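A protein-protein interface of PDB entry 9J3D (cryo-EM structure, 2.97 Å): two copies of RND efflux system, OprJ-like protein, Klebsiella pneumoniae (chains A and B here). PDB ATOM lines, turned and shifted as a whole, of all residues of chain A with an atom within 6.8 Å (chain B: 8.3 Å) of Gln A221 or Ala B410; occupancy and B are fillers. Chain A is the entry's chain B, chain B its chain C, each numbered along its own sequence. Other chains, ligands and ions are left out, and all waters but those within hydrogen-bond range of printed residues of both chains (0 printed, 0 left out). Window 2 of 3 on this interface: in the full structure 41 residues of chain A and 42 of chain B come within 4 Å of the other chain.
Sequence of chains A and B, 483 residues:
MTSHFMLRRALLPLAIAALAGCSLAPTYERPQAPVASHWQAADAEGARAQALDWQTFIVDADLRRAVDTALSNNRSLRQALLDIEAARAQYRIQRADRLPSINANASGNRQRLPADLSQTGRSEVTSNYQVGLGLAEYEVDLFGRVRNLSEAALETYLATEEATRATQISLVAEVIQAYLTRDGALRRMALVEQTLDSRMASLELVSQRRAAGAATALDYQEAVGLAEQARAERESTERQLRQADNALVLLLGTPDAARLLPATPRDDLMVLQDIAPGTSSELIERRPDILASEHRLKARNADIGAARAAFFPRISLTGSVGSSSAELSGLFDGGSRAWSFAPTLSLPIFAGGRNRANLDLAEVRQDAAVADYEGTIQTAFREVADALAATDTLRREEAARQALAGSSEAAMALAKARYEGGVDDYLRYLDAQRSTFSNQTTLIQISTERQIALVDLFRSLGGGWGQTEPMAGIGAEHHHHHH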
ATOM      1  N   LEU A 203     -15.065  -5.895 -22.972  1.00  0.00           N
ATOM      2  CA  LEU A 203     -13.871  -5.964 -23.807  1.00  0.00           C
ATOM      3  C   LEU A 203     -14.136  -5.406 -25.200  1.00  0.00           C
ATOM      4  O   LEU A 203     -13.308  -4.671 -25.748  1.00  0.00           O
ATOM      5  CB  LEU A 203     -13.375  -7.406 -23.896  1.00  0.00           C
ATOM      6  CG  LEU A 203     -12.205  -7.660 -24.846  1.00  0.00           C
ATOM      7  CD1 LEU A 203     -11.035  -6.761 -24.504  1.00  0.00           C
ATOM      8  CD2 LEU A 203     -11.791  -9.122 -24.812  1.00  0.00           C
ATOM      9  N   VAL A 206     -14.340  -1.613 -24.950  1.00  0.00           N
ATOM     10  CA  VAL A 206     -13.035  -0.992 -24.738  1.00  0.00           C
ATOM     11  C   VAL A 206     -12.195  -1.057 -26.007  1.00  0.00           C
ATOM     12  O   VAL A 206     -11.463  -0.115 -26.329  1.00  0.00           O
ATOM     13  CB  VAL A 206     -12.320  -1.649 -23.545  1.00  0.00           C
ATOM     14  CG1 VAL A 206     -10.883  -1.175 -23.456  1.00  0.00           C
ATOM     15  CG2 VAL A 206     -13.054  -1.331 -22.256  1.00  0.00           C
ATOM     16  N   ARG A 210     -10.575   2.216 -27.872  1.00  0.00           N
ATOM     17  CA  ARG A 210      -9.176   2.402 -28.340  1.00  0.00           C
ATOM     18  C   ARG A 210      -9.137   2.584 -29.858  1.00  0.00           C
ATOM     19  O   ARG A 210      -8.352   3.418 -30.289  1.00  0.00           O
ATOM     20  CB  ARG A 210      -8.304   1.217 -27.940  1.00  0.00           C
ATOM     21  CG  ARG A 210      -6.871   1.274 -28.440  1.00  0.00           C
ATOM     22  CD  ARG A 210      -6.371  -0.139 -28.632  1.00  0.00           C
ATOM     23  NE  ARG A 210      -5.087  -0.179 -29.307  1.00  0.00           N
ATOM     24  CZ  ARG A 210      -4.142  -1.077 -29.059  1.00  0.00           C
ATOM     25  NH1 ARG A 210      -4.337  -2.015 -28.148  1.00  0.00           N
ATOM     26  NH2 ARG A 210      -3.004  -1.034 -29.724  1.00  0.00           N
ATOM     27  N   THR A 216      -6.419   4.327 -23.865  1.00  0.00           N
ATOM     28  CA  THR A 216      -5.038   3.900 -23.998  1.00  0.00           C
ATOM     29  C   THR A 216      -4.964   2.388 -24.187  1.00  0.00           C
ATOM     30  O   THR A 216      -5.924   1.653 -23.944  1.00  0.00           O
ATOM     31  CB  THR A 216      -4.225   4.314 -22.773  1.00  0.00           C
ATOM     32  OG1 THR A 216      -4.500   3.414 -21.693  1.00  0.00           O
ATOM     33  CG2 THR A 216      -4.590   5.725 -22.347  1.00  0.00           C
ATOM     34  N   ALA A 217      -3.797   1.920 -24.632  1.00  0.00           N
ATOM     35  CA  ALA A 217      -3.593   0.483 -24.767  1.00  0.00           C
ATOM     36  C   ALA A 217      -3.570  -0.208 -23.411  1.00  0.00           C
ATOM     37  O   ALA A 217      -3.857  -1.406 -23.324  1.00  0.00           O
ATOM     38  CB  ALA A 217      -2.303   0.202 -25.533  1.00  0.00           C
ATOM     39  N   LEU A 218      -3.236   0.525 -22.348  1.00  0.00           N
ATOM     40  CA  LEU A 218      -3.262  -0.052 -21.008  1.00  0.00           C
ATOM     41  C   LEU A 218      -4.676  -0.468 -20.619  1.00  0.00           C
ATOM     42  O   LEU A 218      -4.880  -1.520 -20.003  1.00  0.00           O
ATOM     43  CB  LEU A 218      -2.697   0.949 -20.000  1.00  0.00           C
ATOM     44  CG  LEU A 218      -1.255   1.433 -20.179  1.00  0.00           C
ATOM     45  CD1 LEU A 218      -0.686   1.908 -18.852  1.00  0.00           C
ATOM     46  CD2 LEU A 218      -0.377   0.347 -20.771  1.00  0.00           C
ATOM     47  N   ASP A 219      -5.667   0.358 -20.964  1.00  0.00           N
ATOM     48  CA  ASP A 219      -7.055   0.016 -20.673  1.00  0.00           C
ATOM     49  C   ASP A 219      -7.497  -1.215 -21.454  1.00  0.00           C
ATOM     50  O   ASP A 219      -8.201  -2.082 -20.925  1.00  0.00           O
ATOM     51  CB  ASP A 219      -7.958   1.208 -20.982  1.00  0.00           C
ATOM     52  CG  ASP A 219      -7.509   2.472 -20.274  1.00  0.00           C
ATOM     53  OD1 ASP A 219      -7.166   2.394 -19.076  1.00  0.00           O
ATOM     54  OD2 ASP A 219      -7.497   3.543 -20.916  1.00  0.00           O
ATOM     55  N   TYR A 220      -7.091  -1.311 -22.720  1.00  0.00           N
ATOM     56  CA  TYR A 220      -7.412  -2.499 -23.499  1.00  0.00           C
ATOM     57  C   TYR A 220      -6.767  -3.735 -22.887  1.00  0.00           C
ATOM     58  O   TYR A 220      -7.383  -4.805 -22.822  1.00  0.00           O
ATOM     59  CB  TYR A 220      -6.966  -2.311 -24.949  1.00  0.00           C
ATOM     60  CG  TYR A 220      -7.163  -3.533 -25.815  1.00  0.00           C
ATOM     61  CD1 TYR A 220      -8.386  -3.786 -26.421  1.00  0.00           C
ATOM     62  CD2 TYR A 220      -6.126  -4.427 -26.038  1.00  0.00           C
ATOM     63  CE1 TYR A 220      -8.571  -4.900 -27.213  1.00  0.00           C
ATOM     64  CE2 TYR A 220      -6.303  -5.543 -26.829  1.00  0.00           C
ATOM     65  CZ  TYR A 220      -7.527  -5.773 -27.414  1.00  0.00           C
ATOM     66  OH  TYR A 220      -7.707  -6.884 -28.205  1.00  0.00           O
ATOM     67  N   GLN A 221      -5.524  -3.602 -22.422  1.00  0.00           N
ATOM     68  CA  GLN A 221      -4.848  -4.729 -21.793  1.00  0.00           C
ATOM     69  C   GLN A 221      -5.535  -5.156 -20.503  1.00  0.00           C
ATOM     70  O   GLN A 221      -5.664  -6.357 -20.246  1.00  0.00           O
ATOM     71  CB  GLN A 221      -3.385  -4.387 -21.522  1.00  0.00           C
ATOM     72  CG  GLN A 221      -2.536  -4.238 -22.774  1.00  0.00           C
ATOM     73  CD  GLN A 221      -2.480  -5.504 -23.599  1.00  0.00           C
ATOM     74  OE1 GLN A 221      -2.642  -6.607 -23.079  1.00  0.00           O
ATOM     75  NE2 GLN A 221      -2.250  -5.352 -24.896  1.00  0.00           N
ATOM     76  N   GLU A 222      -5.978  -4.204 -19.678  1.00  0.00           N
ATOM     77  CA  GLU A 222      -6.666  -4.579 -18.445  1.00  0.00           C
ATOM     78  C   GLU A 222      -8.011  -5.232 -18.746  1.00  0.00           C
ATOM     79  O   GLU A 222      -8.419  -6.179 -18.063  1.00  0.00           O
ATOM     80  CB  GLU A 222      -6.802  -3.363 -17.515  1.00  0.00           C
ATOM     81  CG  GLU A 222      -7.697  -2.212 -17.973  1.00  0.00           C
ATOM     82  CD  GLU A 222      -9.178  -2.386 -17.670  1.00  0.00           C
ATOM     83  OE1 GLU A 222      -9.602  -3.484 -17.263  1.00  0.00           O
ATOM     84  OE2 GLU A 222      -9.931  -1.404 -17.847  1.00  0.00           O
ATOM     85  N   ALA A 223      -8.711  -4.751 -19.777  1.00  0.00           N
ATOM     86  CA  ALA A 223      -9.954  -5.406 -20.178  1.00  0.00           C
ATOM     87  C   ALA A 223      -9.696  -6.835 -20.644  1.00  0.00           C
ATOM     88  O   ALA A 223     -10.442  -7.760 -20.292  1.00  0.00           O
ATOM     89  CB  ALA A 223     -10.643  -4.598 -21.274  1.00  0.00           C
ATOM     90  N   VAL A 224      -8.639  -7.032 -21.434  1.00  0.00           N
ATOM     91  CA  VAL A 224      -8.286  -8.373 -21.893  1.00  0.00           C
ATOM     92  C   VAL A 224      -7.969  -9.268 -20.704  1.00  0.00           C
ATOM     93  O   VAL A 224      -8.397 -10.427 -20.643  1.00  0.00           O
ATOM     94  CB  VAL A 224      -7.106  -8.308 -22.880  1.00  0.00           C
ATOM     95  CG1 VAL A 224      -6.491  -9.683 -23.070  1.00  0.00           C
ATOM     96  CG2 VAL A 224      -7.558  -7.743 -24.214  1.00  0.00           C
ATOM     97  N   GLY A 225      -7.209  -8.742 -19.743  1.00  0.00           N
ATOM     98  CA  GLY A 225      -6.872  -9.526 -18.568  1.00  0.00           C
ATOM     99  C   GLY A 225      -8.094  -9.930 -17.769  1.00  0.00           C
ATOM    100  O   GLY A 225      -8.195 -11.068 -17.307  1.00  0.00           O
ATOM    101  N   LEU A 226      -9.040  -9.005 -17.596  1.00  0.00           N
ATOM    102  CA  LEU A 226     -10.264  -9.337 -16.873  1.00  0.00           C
ATOM    103  C   LEU A 226     -11.070 -10.406 -17.603  1.00  0.00           C
ATOM    104  O   LEU A 226     -11.597 -11.336 -16.975  1.00  0.00           O
ATOM    105  CB  LEU A 226     -11.102  -8.079 -16.660  1.00  0.00           C
ATOM    106  CG  LEU A 226     -10.514  -7.070 -15.673  1.00  0.00           C
ATOM    107  CD1 LEU A 226     -11.276  -5.756 -15.725  1.00  0.00           C
ATOM    108  CD2 LEU A 226     -10.513  -7.634 -14.263  1.00  0.00           C
ATOM    109  N   ALA B 403      -2.863 -16.658 -21.803  1.00  0.00           N
ATOM    110  CA  ALA B 403      -3.329 -15.389 -22.358  1.00  0.00           C
ATOM    111  C   ALA B 403      -3.156 -14.255 -21.353  1.00  0.00           C
ATOM    112  O   ALA B 403      -2.733 -13.148 -21.715  1.00  0.00           O
ATOM    113  CB  ALA B 403      -4.788 -15.509 -22.792  1.00  0.00           C
ATOM    114  N   LEU B 404      -3.479 -14.515 -20.085  1.00  0.00           N
ATOM    115  CA  LEU B 404      -3.309 -13.492 -19.054  1.00  0.00           C
ATOM    116  C   LEU B 404      -1.847 -13.083 -18.911  1.00  0.00           C
ATOM    117  O   LEU B 404      -1.535 -11.890 -18.794  1.00  0.00           O
ATOM    118  CB  LEU B 404      -3.855 -13.999 -17.720  1.00  0.00           C
ATOM    119  CG  LEU B 404      -3.622 -13.101 -16.504  1.00  0.00           C
ATOM    120  CD1 LEU B 404      -4.285 -11.748 -16.696  1.00  0.00           C
ATOM    121  CD2 LEU B 404      -4.121 -13.771 -15.234  1.00  0.00           C
ATOM    122  N   ALA B 405      -0.938 -14.059 -18.912  1.00  0.00           N
ATOM    123  CA  ALA B 405       0.484 -13.755 -18.791  1.00  0.00           C
ATOM    124  C   ALA B 405       0.975 -12.945 -19.984  1.00  0.00           C
ATOM    125  O   ALA B 405       1.772 -12.011 -19.832  1.00  0.00           O
ATOM    126  CB  ALA B 405       1.288 -15.046 -18.649  1.00  0.00           C
ATOM    127  N   GLY B 406       0.512 -13.293 -21.185  1.00  0.00           N
ATOM    128  CA  GLY B 406       0.884 -12.518 -22.357  1.00  0.00           C
ATOM    129  C   GLY B 406       0.393 -11.085 -22.287  1.00  0.00           C
ATOM    130  O   GLY B 406       1.112 -10.150 -22.653  1.00  0.00           O
ATOM    131  N   SER B 407      -0.842 -10.890 -21.816  1.00  0.00           N
ATOM    132  CA  SER B 407      -1.361  -9.536 -21.657  1.00  0.00           C
ATOM    133  C   SER B 407      -0.546  -8.750 -20.638  1.00  0.00           C
ATOM    134  O   SER B 407      -0.251  -7.564 -20.842  1.00  0.00           O
ATOM    135  CB  SER B 407      -2.830  -9.581 -21.247  1.00  0.00           C
ATOM    136  OG  SER B 407      -3.350  -8.274 -21.085  1.00  0.00           O
ATOM    137  N   SER B 408      -0.169  -9.395 -19.534  1.00  0.00           N
ATOM    138  CA  SER B 408       0.652  -8.715 -18.538  1.00  0.00           C
ATOM    139  C   SER B 408       2.021  -8.353 -19.103  1.00  0.00           C
ATOM    140  O   SER B 408       2.569  -7.296 -18.781  1.00  0.00           O
ATOM    141  CB  SER B 408       0.793  -9.582 -17.289  1.00  0.00           C
ATOM    142  OG  SER B 408       1.305 -10.860 -17.614  1.00  0.00           O
ATOM    143  N   GLU B 409       2.584  -9.210 -19.956  1.00  0.00           N
ATOM    144  CA  GLU B 409       3.878  -8.905 -20.562  1.00  0.00           C
ATOM    145  C   GLU B 409       3.765  -7.754 -21.560  1.00  0.00           C
ATOM    146  O   GLU B 409       4.685  -6.938 -21.700  1.00  0.00           O
ATOM    147  CB  GLU B 409       4.444 -10.155 -21.237  1.00  0.00           C
ATOM    148  CG  GLU B 409       5.677 -10.750 -20.563  1.00  0.00           C
ATOM    149  CD  GLU B 409       6.853  -9.791 -20.470  1.00  0.00           C
ATOM    150  OE1 GLU B 409       6.869  -8.772 -21.192  1.00  0.00           O
ATOM    151  OE2 GLU B 409       7.771 -10.063 -19.670  1.00  0.00           O
ATOM    152  N   ALA B 410       2.646  -7.684 -22.283  1.00  0.00           N
ATOM    153  CA  ALA B 410       2.426  -6.538 -23.163  1.00  0.00           C
ATOM    154  C   ALA B 410       2.322  -5.248 -22.357  1.00  0.00           C
ATOM    155  O   ALA B 410       2.874  -4.207 -22.746  1.00  0.00           O
ATOM    156  CB  ALA B 410       1.170  -6.754 -24.005  1.00  0.00           C
ATOM    157  N   ALA B 411       1.618  -5.303 -21.225  1.00  0.00           N
ATOM    158  CA  ALA B 411       1.578  -4.154 -20.327  1.00  0.00           C
ATOM    159  C   ALA B 411       2.973  -3.811 -19.816  1.00  0.00           C
ATOM    160  O   ALA B 411       3.300  -2.635 -19.632  1.00  0.00           O
ATOM    161  CB  ALA B 411       0.624  -4.426 -19.165  1.00  0.00           C
ATOM    162  N   MET B 412       3.800  -4.829 -19.565  1.00  0.00           N
ATOM    163  CA  MET B 412       5.210  -4.602 -19.246  1.00  0.00           C
ATOM    164  C   MET B 412       5.901  -3.777 -20.314  1.00  0.00           C
ATOM    165  O   MET B 412       6.567  -2.782 -20.006  1.00  0.00           O
ATOM    166  CB  MET B 412       5.938  -5.941 -19.084  1.00  0.00           C
ATOM    167  CG  MET B 412       7.208  -6.000 -18.205  1.00  0.00           C
ATOM    168  SD  MET B 412       7.526  -4.822 -16.887  1.00  0.00           S
ATOM    169  CE  MET B 412       5.996  -4.937 -16.027  1.00  0.00           C
ATOM    170  N   ALA B 413       5.788  -4.201 -21.571  1.00  0.00           N
ATOM    171  CA  ALA B 413       6.472  -3.488 -22.644  1.00  0.00           C
ATOM    172  C   ALA B 413       6.011  -2.039 -22.708  1.00  0.00           C
ATOM    173  O   ALA B 413       6.833  -1.118 -22.802  1.00  0.00           O
ATOM    174  CB  ALA B 413       6.236  -4.188 -23.982  1.00  0.00           C
ATOM    175  N   LEU B 414       4.698  -1.818 -22.616  1.00  0.00           N
ATOM    176  CA  LEU B 414       4.176  -0.456 -22.691  1.00  0.00           C
ATOM    177  C   LEU B 414       4.639   0.396 -21.513  1.00  0.00           C
ATOM    178  O   LEU B 414       5.053   1.547 -21.700  1.00  0.00           O
ATOM    179  CB  LEU B 414       2.653  -0.491 -22.768  1.00  0.00           C
ATOM    180  CG  LEU B 414       2.119  -1.078 -24.072  1.00  0.00           C
ATOM    181  CD1 LEU B 414       0.616  -1.238 -24.009  1.00  0.00           C
ATOM    182  CD2 LEU B 414       2.520  -0.211 -25.249  1.00  0.00           C
ATOM    183  N   ALA B 415       4.584  -0.147 -20.294  1.00  0.00           N
ATOM    184  CA  ALA B 415       4.985   0.626 -19.122  1.00  0.00           C
ATOM    185  C   ALA B 415       6.474   0.939 -19.147  1.00  0.00           C
ATOM    186  O   ALA B 415       6.889   2.044 -18.781  1.00  0.00           O
ATOM    187  CB  ALA B 415       4.614  -0.126 -17.846  1.00  0.00           C
ATOM    188  N   LYS B 416       7.297  -0.026 -19.562  1.00  0.00           N
ATOM    189  CA  LYS B 416       8.731   0.217 -19.663  1.00  0.00           C
ATOM    190  C   LYS B 416       9.021   1.291 -20.701  1.00  0.00           C
ATOM    191  O   LYS B 416       9.866   2.167 -20.485  1.00  0.00           O
ATOM    192  CB  LYS B 416       9.458  -1.090 -19.998  1.00  0.00           C
ATOM    193  CG  LYS B 416      10.986  -1.028 -19.970  1.00  0.00           C
ATOM    194  CD  LYS B 416      11.587  -0.543 -21.283  1.00  0.00           C
ATOM    195  CE  LYS B 416      13.093  -0.745 -21.318  1.00  0.00           C
ATOM    196  NZ  LYS B 416      13.456  -2.181 -21.466  1.00  0.00           N
ATOM    197  N   ALA B 417       8.329   1.236 -21.842  1.00  0.00           N
ATOM    198  CA  ALA B 417       8.525   2.256 -22.864  1.00  0.00           C
ATOM    199  C   ALA B 417       8.122   3.632 -22.354  1.00  0.00           C
ATOM    200  O   ALA B 417       8.800   4.628 -22.630  1.00  0.00           O
ATOM    201  CB  ALA B 417       7.740   1.894 -24.122  1.00  0.00           C
ATOM    202  N   ALA B 432       3.862  -2.524 -12.276  1.00  0.00           N
ATOM    203  CA  ALA B 432       3.592  -3.392 -13.413  1.00  0.00           C
ATOM    204  C   ALA B 432       4.444  -4.655 -13.343  1.00  0.00           C
ATOM    205  O   ALA B 432       3.979  -5.746 -13.695  1.00  0.00           O
ATOM    206  CB  ALA B 432       3.830  -2.630 -14.715  1.00  0.00           C
ATOM    207  N   THR B 436       2.743  -8.354 -13.406  1.00  0.00           N
ATOM    208  CA  THR B 436       3.029  -9.360 -14.422  1.00  0.00           C
ATOM    209  C   THR B 436       3.664 -10.594 -13.798  1.00  0.00           C
ATOM    210  O   THR B 436       3.395 -11.724 -14.219  1.00  0.00           O
ATOM    211  CB  THR B 436       3.916  -8.783 -15.531  1.00  0.00           C
ATOM    212  OG1 THR B 436       4.090  -9.766 -16.559  1.00  0.00           O
ATOM    213  CG2 THR B 436       5.280  -8.381 -15.006  1.00  0.00           C
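The side-chain hydroxyl (OG) of Ser B407 is in hydrogen-bond range of the side-chain amide oxygen (OE1) of Gln A221 (2.7 Å).
OG1 of Thr A216 sits close to N of Leu A218. The backbone carbonyl oxygen of Leu B404 lies within hydrogen-bond range of the side-chain hydroxyl of Ser B408, at 3.2 Å.
Of chain B, only Ser B407 (2.7 Å) and Ala B410 (3.8 Å) come within 4 Å of Gln A221. Of chain A, only Gln A221 (3.8 Å) comes within 4 Å of Ala B410. Of the printed residues of chain B, Ala A217 touches Leu B414 (3.6 Å). Printed residues of chain A within 4 Å of Ser B407: Gln A221 (2.7 Å) and Val A224 (3.97 Å). Printed residues of chain A within 4 Å of Leu B404: Gly A225 (3.9 Å). Printed residues of chain B within 4 Å of Gly A225: Leu B404. Printed residues of chain B within 4 Å of Val A224: Ser B407 (3.97 Å). Ala B411 touches none of the printed residues of chain A. Ala A223 touches none of the printed residues of chain B. The nearest printed residue of chain A that does not touch Leu B414 is Gln A221 (4.5 Å).
Ala A217 touches Leu B414. Leu A218 touches Leu B414. Gln A221 touches Ala B410. CG1 of Val A224 touches OG of Ser B407, at 3.97 Å. Gly A225 touches Leu B404.
No position is printed for both chains. Of the 6 pairs that touch across the chains among the printed residues, none has its exchanged pair printed and touching as well.
Of the 14 printed residues of chain A, 5 touch a printed residue of chain B. Of the 17 printed residues of chain B, 4 touch a printed residue of chain A. Printed residues of chain B that touch a printed residue of chain A: Leu B404, Ser B407, Ala B410 and Leu B414. Hydrophobic or aromatic side chains of chain B within 4 Å of the printed part of chain A: Leu B404, Ala B410 and Leu B414. Among the printed residues, 6 pairs touch across the chains.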
